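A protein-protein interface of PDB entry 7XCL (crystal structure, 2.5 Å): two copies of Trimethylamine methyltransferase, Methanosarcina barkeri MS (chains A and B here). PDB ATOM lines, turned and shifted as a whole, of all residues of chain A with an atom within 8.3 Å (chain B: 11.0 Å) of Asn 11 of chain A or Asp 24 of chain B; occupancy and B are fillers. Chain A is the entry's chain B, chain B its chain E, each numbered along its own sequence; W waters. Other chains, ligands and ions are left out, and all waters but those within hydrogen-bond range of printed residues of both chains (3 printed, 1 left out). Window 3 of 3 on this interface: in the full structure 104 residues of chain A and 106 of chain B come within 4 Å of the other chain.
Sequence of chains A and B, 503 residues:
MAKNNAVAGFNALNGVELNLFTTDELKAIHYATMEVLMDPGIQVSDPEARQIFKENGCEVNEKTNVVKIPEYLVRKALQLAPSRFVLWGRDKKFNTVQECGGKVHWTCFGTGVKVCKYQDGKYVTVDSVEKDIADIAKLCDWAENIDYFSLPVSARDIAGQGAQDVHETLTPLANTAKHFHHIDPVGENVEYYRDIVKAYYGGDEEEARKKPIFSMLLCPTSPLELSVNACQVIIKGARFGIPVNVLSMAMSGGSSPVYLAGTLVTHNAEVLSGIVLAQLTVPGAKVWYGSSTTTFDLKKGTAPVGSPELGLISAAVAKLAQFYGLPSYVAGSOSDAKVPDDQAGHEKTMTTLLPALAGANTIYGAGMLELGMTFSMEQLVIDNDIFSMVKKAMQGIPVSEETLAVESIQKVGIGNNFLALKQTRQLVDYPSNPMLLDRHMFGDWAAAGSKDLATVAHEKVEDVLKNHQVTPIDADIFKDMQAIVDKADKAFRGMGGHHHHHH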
ATOM      1  N   ALA A   8      -5.364 -37.716  14.419  1.00  0.00           N
ATOM      2  CA  ALA A   8      -4.286 -37.228  13.556  1.00  0.00           C
ATOM      3  C   ALA A   8      -3.351 -36.260  14.293  1.00  0.00           C
ATOM      4  O   ALA A   8      -3.702 -35.728  15.346  1.00  0.00           O
ATOM      5  CB  ALA A   8      -4.875 -36.544  12.328  1.00  0.00           C
ATOM      6  N   GLY A   9      -2.164 -36.040  13.723  1.00  0.00           N
ATOM      7  CA  GLY A   9      -1.183 -35.143  14.313  1.00  0.00           C
ATOM      8  C   GLY A   9      -1.814 -33.954  15.014  1.00  0.00           C
ATOM      9  O   GLY A   9      -2.654 -33.257  14.444  1.00  0.00           O
ATOM     10  N   PHE A  10      -1.371 -33.712  16.242  1.00  0.00           N
ATOM     11  CA  PHE A  10      -1.900 -32.648  17.095  1.00  0.00           C
ATOM     12  C   PHE A  10      -0.754 -31.802  17.696  1.00  0.00           C
ATOM     13  O   PHE A  10       0.229 -32.359  18.187  1.00  0.00           O
ATOM     14  CB  PHE A  10      -2.696 -33.339  18.205  1.00  0.00           C
ATOM     15  CG  PHE A  10      -3.464 -32.422  19.079  1.00  0.00           C
ATOM     16  CD1 PHE A  10      -4.731 -31.979  18.699  1.00  0.00           C
ATOM     17  CD2 PHE A  10      -2.949 -32.026  20.306  1.00  0.00           C
ATOM     18  CE1 PHE A  10      -5.486 -31.149  19.538  1.00  0.00           C
ATOM     19  CE2 PHE A  10      -3.687 -31.200  21.153  1.00  0.00           C
ATOM     20  CZ  PHE A  10      -4.963 -30.760  20.768  1.00  0.00           C
ATOM     21  N   ASN A  11      -0.875 -30.472  17.655  1.00  0.00           N
ATOM     22  CA  ASN A  11       0.153 -29.579  18.227  1.00  0.00           C
ATOM     23  C   ASN A  11      -0.194 -29.198  19.670  1.00  0.00           C
ATOM     24  O   ASN A  11      -1.264 -28.642  19.936  1.00  0.00           O
ATOM     25  CB  ASN A  11       0.277 -28.304  17.408  1.00  0.00           C
ATOM     26  CG  ASN A  11       0.677 -28.574  15.986  1.00  0.00           C
ATOM     27  OD1 ASN A  11       1.818 -28.948  15.705  1.00  0.00           O
ATOM     28  ND2 ASN A  11      -0.267 -28.395  15.067  1.00  0.00           N
ATOM     29  N   ALA A  12       0.718 -29.472  20.599  1.00  0.00           N
ATOM     30  CA  ALA A  12       0.446 -29.191  22.001  1.00  0.00           C
ATOM     31  C   ALA A  12       1.439 -28.293  22.706  1.00  0.00           C
ATOM     32  O   ALA A  12       2.578 -28.135  22.280  1.00  0.00           O
ATOM     33  CB  ALA A  12       0.335 -30.501  22.767  1.00  0.00           C
ATOM     34  N   LEU A  13       0.978 -27.716  23.807  1.00  0.00           N
ATOM     35  CA  LEU A  13       1.812 -26.865  24.628  1.00  0.00           C
ATOM     36  C   LEU A  13       1.778 -27.387  26.063  1.00  0.00           C
ATOM     37  O   LEU A  13       0.769 -27.262  26.838  1.00  0.00           O
ATOM     38  CB  LEU A  13       1.364 -25.404  24.552  1.00  0.00           C
ATOM     39  CG  LEU A  13       2.192 -24.435  25.407  1.00  0.00           C
ATOM     40  CD1 LEU A  13       3.660 -24.768  25.297  1.00  0.00           C
ATOM     41  CD2 LEU A  13       1.936 -23.009  24.965  1.00  0.00           C
ATOM     42  N   ASN A  14       2.902 -28.021  26.381  1.00  0.00           N
ATOM     43  CA  ASN A  14       3.131 -28.609  27.678  1.00  0.00           C
ATOM     44  C   ASN A  14       3.868 -27.605  28.534  1.00  0.00           C
ATOM     45  O   ASN A  14       4.972 -27.186  28.200  1.00  0.00           O
ATOM     46  CB  ASN A  14       3.952 -29.894  27.533  1.00  0.00           C
ATOM     47  CG  ASN A  14       3.248 -30.941  26.679  1.00  0.00           C
ATOM     48  OD1 ASN A  14       2.043 -31.175  26.830  1.00  0.00           O
ATOM     49  ND2 ASN A  14       3.997 -31.582  25.785  1.00  0.00           N
ATOM     50  N   VAL A 399      -3.822 -30.308  28.097  1.00  0.00           N
ATOM     51  CA  VAL A 399      -5.071 -30.523  27.384  1.00  0.00           C
ATOM     52  C   VAL A 399      -5.078 -31.890  26.706  1.00  0.00           C
ATOM     53  O   VAL A 399      -4.250 -32.164  25.839  1.00  0.00           O
ATOM     54  CB  VAL A 399      -5.301 -29.449  26.312  1.00  0.00           C
ATOM     55  CG1 VAL A 399      -6.548 -29.785  25.503  1.00  0.00           C
ATOM     56  CG2 VAL A 399      -5.457 -28.094  26.965  1.00  0.00           C
ATOM     57  N   LEU A 404      -9.942 -32.915  29.762  1.00  0.00           N
ATOM     58  CA  LEU A 404     -11.120 -32.126  29.409  1.00  0.00           C
ATOM     59  C   LEU A 404     -12.297 -32.681  30.219  1.00  0.00           C
ATOM     60  O   LEU A 404     -13.226 -31.951  30.581  1.00  0.00           O
ATOM     61  CB  LEU A 404     -11.394 -32.216  27.911  1.00  0.00           C
ATOM     62  CG  LEU A 404     -10.367 -31.411  27.110  1.00  0.00           C
ATOM     63  CD1 LEU A 404     -10.445 -31.782  25.649  1.00  0.00           C
ATOM     64  CD2 LEU A 404     -10.614 -29.915  27.310  1.00  0.00           C
ATOM     65  N   LEU B  20       0.060 -20.477  26.828  1.00  0.00           N
ATOM     66  CA  LEU B  20      -0.525 -21.634  27.484  1.00  0.00           C
ATOM     67  C   LEU B  20      -1.195 -22.628  26.548  1.00  0.00           C
ATOM     68  O   LEU B  20      -1.383 -23.780  26.921  1.00  0.00           O
ATOM     69  CB  LEU B  20      -1.550 -21.178  28.512  1.00  0.00           C
ATOM     70  CG  LEU B  20      -0.978 -20.494  29.741  1.00  0.00           C
ATOM     71  CD1 LEU B  20      -2.126 -19.998  30.615  1.00  0.00           C
ATOM     72  CD2 LEU B  20      -0.086 -21.481  30.491  1.00  0.00           C
ATOM     73  N   PHE B  21      -1.547 -22.193  25.339  1.00  0.00           N
ATOM     74  CA  PHE B  21      -2.244 -23.070  24.402  1.00  0.00           C
ATOM     75  C   PHE B  21      -1.861 -22.892  22.949  1.00  0.00           C
ATOM     76  O   PHE B  21      -1.481 -21.806  22.521  1.00  0.00           O
ATOM     77  CB  PHE B  21      -3.759 -22.820  24.432  1.00  0.00           C
ATOM     78  CG  PHE B  21      -4.376 -22.855  25.790  1.00  0.00           C
ATOM     79  CD1 PHE B  21      -4.607 -24.068  26.437  1.00  0.00           C
ATOM     80  CD2 PHE B  21      -4.789 -21.670  26.401  1.00  0.00           C
ATOM     81  CE1 PHE B  21      -5.250 -24.101  27.672  1.00  0.00           C
ATOM     82  CE2 PHE B  21      -5.433 -21.697  27.640  1.00  0.00           C
ATOM     83  CZ  PHE B  21      -5.664 -22.913  28.275  1.00  0.00           C
ATOM     84  N   THR B  22      -2.015 -23.971  22.190  1.00  0.00           N
ATOM     85  CA  THR B  22      -1.798 -23.937  20.753  1.00  0.00           C
ATOM     86  C   THR B  22      -3.232 -23.711  20.266  1.00  0.00           C
ATOM     87  O   THR B  22      -4.188 -23.879  21.034  1.00  0.00           O
ATOM     88  CB  THR B  22      -1.320 -25.294  20.185  1.00  0.00           C
ATOM     89  OG1 THR B  22      -2.263 -26.318  20.536  1.00  0.00           O
ATOM     90  CG2 THR B  22       0.058 -25.652  20.716  1.00  0.00           C
ATOM     91  N   THR B  23      -3.395 -23.324  19.007  1.00  0.00           N
ATOM     92  CA  THR B  23      -4.732 -23.118  18.492  1.00  0.00           C
ATOM     93  C   THR B  23      -5.517 -24.430  18.612  1.00  0.00           C
ATOM     94  O   THR B  23      -6.680 -24.424  19.027  1.00  0.00           O
ATOM     95  CB  THR B  23      -4.681 -22.638  17.035  1.00  0.00           C
ATOM     96  OG1 THR B  23      -4.213 -21.285  17.006  1.00  0.00           O
ATOM     97  CG2 THR B  23      -6.050 -22.695  16.401  1.00  0.00           C
ATOM     98  N   ASP B  24      -4.875 -25.550  18.276  1.00  0.00           N
ATOM     99  CA  ASP B  24      -5.519 -26.861  18.368  1.00  0.00           C
ATOM    100  C   ASP B  24      -6.115 -27.086  19.742  1.00  0.00           C
ATOM    101  O   ASP B  24      -7.221 -27.611  19.867  1.00  0.00           O
ATOM    102  CB  ASP B  24      -4.528 -28.004  18.110  1.00  0.00           C
ATOM    103  CG  ASP B  24      -4.124 -28.126  16.653  1.00  0.00           C
ATOM    104  OD1 ASP B  24      -4.922 -27.725  15.777  1.00  0.00           O
ATOM    105  OD2 ASP B  24      -3.011 -28.643  16.390  1.00  0.00           O
ATOM    106  N   GLU B  25      -5.373 -26.698  20.777  1.00  0.00           N
ATOM    107  CA  GLU B  25      -5.829 -26.894  22.145  1.00  0.00           C
ATOM    108  C   GLU B  25      -6.985 -25.980  22.492  1.00  0.00           C
ATOM    109  O   GLU B  25      -7.905 -26.385  23.204  1.00  0.00           O
ATOM    110  CB  GLU B  25      -4.660 -26.713  23.118  1.00  0.00           C
ATOM    111  CG  GLU B  25      -3.580 -27.776  22.924  1.00  0.00           C
ATOM    112  CD  GLU B  25      -2.317 -27.520  23.723  1.00  0.00           C
ATOM    113  OE1 GLU B  25      -1.832 -26.370  23.716  1.00  0.00           O
ATOM    114  OE2 GLU B  25      -1.795 -28.473  24.341  1.00  0.00           O
ATOM    115  N   LEU B  26      -6.952 -24.753  21.984  1.00  0.00           N
ATOM    116  CA  LEU B  26      -8.041 -23.823  22.245  1.00  0.00           C
ATOM    117  C   LEU B  26      -9.311 -24.402  21.630  1.00  0.00           C
ATOM    118  O   LEU B  26     -10.363 -24.437  22.266  1.00  0.00           O
ATOM    119  CB  LEU B  26      -7.741 -22.452  21.639  1.00  0.00           C
ATOM    120  CG  LEU B  26      -6.826 -21.541  22.465  1.00  0.00           C
ATOM    121  CD1 LEU B  26      -6.528 -20.254  21.695  1.00  0.00           C
ATOM    122  CD2 LEU B  26      -7.500 -21.216  23.795  1.00  0.00           C
ATOM    123  N   LYS B  27      -9.205 -24.876  20.395  1.00  0.00           N
ATOM    124  CA  LYS B  27     -10.353 -25.453  19.717  1.00  0.00           C
ATOM    125  C   LYS B  27     -10.912 -26.644  20.487  1.00  0.00           C
ATOM    126  O   LYS B  27     -12.127 -26.820  20.572  1.00  0.00           O
ATOM    127  CB  LYS B  27      -9.977 -25.878  18.297  1.00  0.00           C
ATOM    128  CG  LYS B  27      -9.752 -24.713  17.335  1.00  0.00           C
ATOM    129  CD  LYS B  27      -9.449 -25.229  15.934  1.00  0.00           C
ATOM    130  CE  LYS B  27      -9.088 -24.102  14.980  1.00  0.00           C
ATOM    131  NZ  LYS B  27      -8.733 -24.608  13.621  1.00  0.00           N
ATOM    132  N   ALA B  28     -10.027 -27.457  21.054  1.00  0.00           N
ATOM    133  CA  ALA B  28     -10.457 -28.627  21.813  1.00  0.00           C
ATOM    134  C   ALA B  28     -11.345 -28.218  22.978  1.00  0.00           C
ATOM    135  O   ALA B  28     -12.359 -28.861  23.257  1.00  0.00           O
ATOM    136  CB  ALA B  28      -9.245 -29.403  22.327  1.00  0.00           C
ATOM    137  N   ILE B  29     -10.964 -27.145  23.657  1.00  0.00           N
ATOM    138  CA  ILE B  29     -11.742 -26.671  24.787  1.00  0.00           C
ATOM    139  C   ILE B  29     -13.103 -26.193  24.304  1.00  0.00           C
ATOM    140  O   ILE B  29     -14.127 -26.468  24.934  1.00  0.00           O
ATOM    141  CB  ILE B  29     -11.006 -25.535  25.520  1.00  0.00           C
ATOM    142  CG1 ILE B  29      -9.730 -26.094  26.154  1.00  0.00           C
ATOM    143  CG2 ILE B  29     -11.901 -24.928  26.600  1.00  0.00           C
ATOM    144  CD1 ILE B  29      -8.904 -25.066  26.872  1.00  0.00           C
ATOM    145  N   HIS B  30     -13.108 -25.494  23.174  1.00  0.00           N
ATOM    146  CA  HIS B  30     -14.338 -24.976  22.590  1.00  0.00           C
ATOM    147  C   HIS B  30     -15.309 -26.108  22.256  1.00  0.00           C
ATOM    148  O   HIS B  30     -16.483 -26.048  22.616  1.00  0.00           O
ATOM    149  CB  HIS B  30     -14.030 -24.184  21.319  1.00  0.00           C
ATOM    150  CG  HIS B  30     -15.252 -23.677  20.623  1.00  0.00           C
ATOM    151  ND1 HIS B  30     -16.056 -22.689  21.154  1.00  0.00           N
ATOM    152  CD2 HIS B  30     -15.843 -24.066  19.466  1.00  0.00           C
ATOM    153  CE1 HIS B  30     -17.092 -22.496  20.356  1.00  0.00           C
ATOM    154  NE2 HIS B  30     -16.987 -23.320  19.327  1.00  0.00           N
ATOM    155  N   TYR B  31     -14.821 -27.133  21.558  1.00  0.00           N
ATOM    156  CA  TYR B  31     -15.661 -28.274  21.193  1.00  0.00           C
ATOM    157  C   TYR B  31     -16.289 -28.924  22.425  1.00  0.00           C
ATOM    158  O   TYR B  31     -17.487 -29.213  22.441  1.00  0.00           O
ATOM    159  CB  TYR B  31     -14.854 -29.333  20.434  1.00  0.00           C
ATOM    160  CG  TYR B  31     -14.288 -28.866  19.113  1.00  0.00           C
ATOM    161  CD1 TYR B  31     -15.015 -28.018  18.278  1.00  0.00           C
ATOM    162  CD2 TYR B  31     -13.018 -29.261  18.704  1.00  0.00           C
ATOM    163  CE1 TYR B  31     -14.485 -27.571  17.073  1.00  0.00           C
ATOM    164  CE2 TYR B  31     -12.481 -28.822  17.500  1.00  0.00           C
ATOM    165  CZ  TYR B  31     -13.217 -27.977  16.692  1.00  0.00           C
ATOM    166  OH  TYR B  31     -12.673 -27.530  15.510  1.00  0.00           O
ATOM    167  N   ALA B  32     -15.478 -29.157  23.452  1.00  0.00           N
ATOM    168  CA  ALA B  32     -15.975 -29.772  24.674  1.00  0.00           C
ATOM    169  C   ALA B  32     -17.082 -28.917  25.270  1.00  0.00           C
ATOM    170  O   ALA B  32     -18.097 -29.438  25.734  1.00  0.00           O
ATOM    171  CB  ALA B  32     -14.840 -29.945  25.687  1.00  0.00           C
ATOM    172  N   ALA B 261      -8.181 -28.262  32.816  1.00  0.00           N
ATOM    173  CA  ALA B 261      -8.808 -28.236  31.491  1.00  0.00           C
ATOM    174  C   ALA B 261     -10.325 -28.410  31.631  1.00  0.00           C
ATOM    175  O   ALA B 261     -11.108 -27.584  31.163  1.00  0.00           O
ATOM    176  CB  ALA B 261      -8.239 -29.344  30.616  1.00  0.00           C
ATOM    177  N   LEU B 320      -8.517 -17.395  26.676  1.00  0.00           N
ATOM    178  CA  LEU B 320      -9.787 -17.799  26.090  1.00  0.00           C
ATOM    179  C   LEU B 320     -10.562 -16.562  25.659  1.00  0.00           C
ATOM    180  O   LEU B 320     -11.162 -16.539  24.584  1.00  0.00           O
ATOM    181  CB  LEU B 320     -10.602 -18.624  27.088  1.00  0.00           C
ATOM    182  CG  LEU B 320     -10.186 -20.092  27.232  1.00  0.00           C
ATOM    183  CD1 LEU B 320     -10.899 -20.717  28.410  1.00  0.00           C
ATOM    184  CD2 LEU B 320     -10.526 -20.845  25.960  1.00  0.00           C
ATOM    185  N   PHE B 323      -9.083 -15.391  22.551  1.00  0.00           N
ATOM    186  CA  PHE B 323      -9.453 -16.310  21.490  1.00  0.00           C
ATOM    187  C   PHE B 323     -10.873 -15.989  21.000  1.00  0.00           C
ATOM    188  O   PHE B 323     -11.146 -16.014  19.798  1.00  0.00           O
ATOM    189  CB  PHE B 323      -9.395 -17.726  22.051  1.00  0.00           C
ATOM    190  CG  PHE B 323      -9.944 -18.778  21.138  1.00  0.00           C
ATOM    191  CD1 PHE B 323      -9.288 -19.111  19.959  1.00  0.00           C
ATOM    192  CD2 PHE B 323     -11.066 -19.506  21.510  1.00  0.00           C
ATOM    193  CE1 PHE B 323      -9.734 -20.166  19.167  1.00  0.00           C
ATOM    194  CE2 PHE B 323     -11.523 -20.564  20.726  1.00  0.00           C
ATOM    195  CZ  PHE B 323     -10.853 -20.896  19.553  1.00  0.00           C
ATOM    196  N   TYR B 324     -11.766 -15.668  21.935  1.00  0.00           N
ATOM    197  CA  TYR B 324     -13.159 -15.378  21.604  1.00  0.00           C
ATOM    198  C   TYR B 324     -13.449 -13.951  21.164  1.00  0.00           C
ATOM    199  O   TYR B 324     -14.501 -13.687  20.585  1.00  0.00           O
ATOM    200  CB  TYR B 324     -14.071 -15.758  22.776  1.00  0.00           C
ATOM    201  CG  TYR B 324     -14.274 -17.250  22.932  1.00  0.00           C
ATOM    202  CD1 TYR B 324     -14.585 -18.049  21.828  1.00  0.00           C
ATOM    203  CD2 TYR B 324     -14.199 -17.862  24.186  1.00  0.00           C
ATOM    204  CE1 TYR B 324     -14.824 -19.419  21.966  1.00  0.00           C
ATOM    205  CE2 TYR B 324     -14.436 -19.237  24.340  1.00  0.00           C
ATOM    206  CZ  TYR B 324     -14.751 -20.006  23.224  1.00  0.00           C
ATOM    207  OH  TYR B 324     -15.030 -21.350  23.363  1.00  0.00           O
HETATM  208  O   HOH W   1      -2.280 -31.181  24.068  1.00  0.00           O
HETATM  209  O   HOH W   2      -1.346 -29.534  27.041  1.00  0.00           O
HETATM  210  O   HOH W   3      -0.345 -25.214  29.014  1.00  0.00           O
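N of Thr 22 of chain B lies within hydrogen-bond range of OE1 of Glu 25 of chain B.
Phe 10 of chain A touches two residues of chain B. Printed residues of chain B within 4 Å of Ala 12 of chain A: Thr 22 and Glu 25. Printed residues of chain B within 4 Å of Leu 13 of chain A: Leu 20, Phe 21, Thr 22 and Glu 25. Of the printed residues of chain A, Phe 21 of chain B touches Leu 13. Printed residues of chain A within 4 Å of Thr 22 of chain B: Asn 11 (2.6 Å), Ala 12 (3.6 Å) and Leu 13 (3.8 Å). Of the printed residues of chain A, Glu 25 of chain B touches Phe 10 (3.9 Å), Asn 11 (3.9 Å), Ala 12 (3.3 Å) and Leu 13 (2.9 Å). Tyr 324 of chain B touches none of the printed residues of chain A. The nearest residue of chain B that does not touch Asn 11 of chain A is Thr 23 of chain B (5.8 Å). The nearest printed residue of chain A that does not touch Leu 20 of chain B is Val 399 of chain A (5.9 Å).
Water W3 lies within hydrogen-bond range of O of Leu 20 of chain B (2.7 Å) and O of Leu 13 of chain A (3.2 Å). Water W1 bridges the side-chain carboxylate (OE2) of Glu 25 of chain B (2.8 Å) and the backbone carbonyl oxygen (O) of Val 399 of chain A (2.8 Å). Water W2 lies within hydrogen-bond range of the backbone NH of Val 399 of chain A, the side-chain carboxylate of Glu 25 of chain B and the backbone carbonyl oxygen of Leu 13 of chain A.
Among the printed residues, pairs that only touch across the chains: Phe 10 of chain A with Asp 24 of chain B (3.6 Å), Phe 10 of chain A with Glu 25 of chain B (3.9 Å), Asn 11 of chain A with Glu 25 of chain B (3.9 Å), Ala 12 of chain A with Thr 22 of chain B (3.6 Å), Ala 12 of chain A with Glu 25 of chain B (3.3 Å), Leu 13 of chain A with Leu 20 of chain B (3.5 Å), Leu 13 of chain A with Phe 21 of chain B (3.6 Å) and Leu 13 of chain A with Thr 22 of chain B (3.8 Å).
OG1 of Thr 22 of chain B sits at hydrogen-bond distance from O of Asn 11 of chain A, 2.6 Å away. The side-chain amide nitrogen (ND2) of Asn 11 of chain A is in hydrogen-bond range of the side-chain carboxylate (OD2) of Asp 24 of chain B (3.1 Å). The backbone NH of Leu 13 of chain A is in hydrogen-bond range of the side-chain carboxylate of Glu 25 of chain B (2.9 Å).
No position is printed for both chains.
Along chain B the printed residues that touch a printed residue of chain A span positions 20 to 25. Hydrophobic or aromatic side chains of chain A within 4 Å of the printed part of chain B: Phe 10, Ala 12 and Leu 13. Among the printed residues, 11 pairs touch across the chains.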
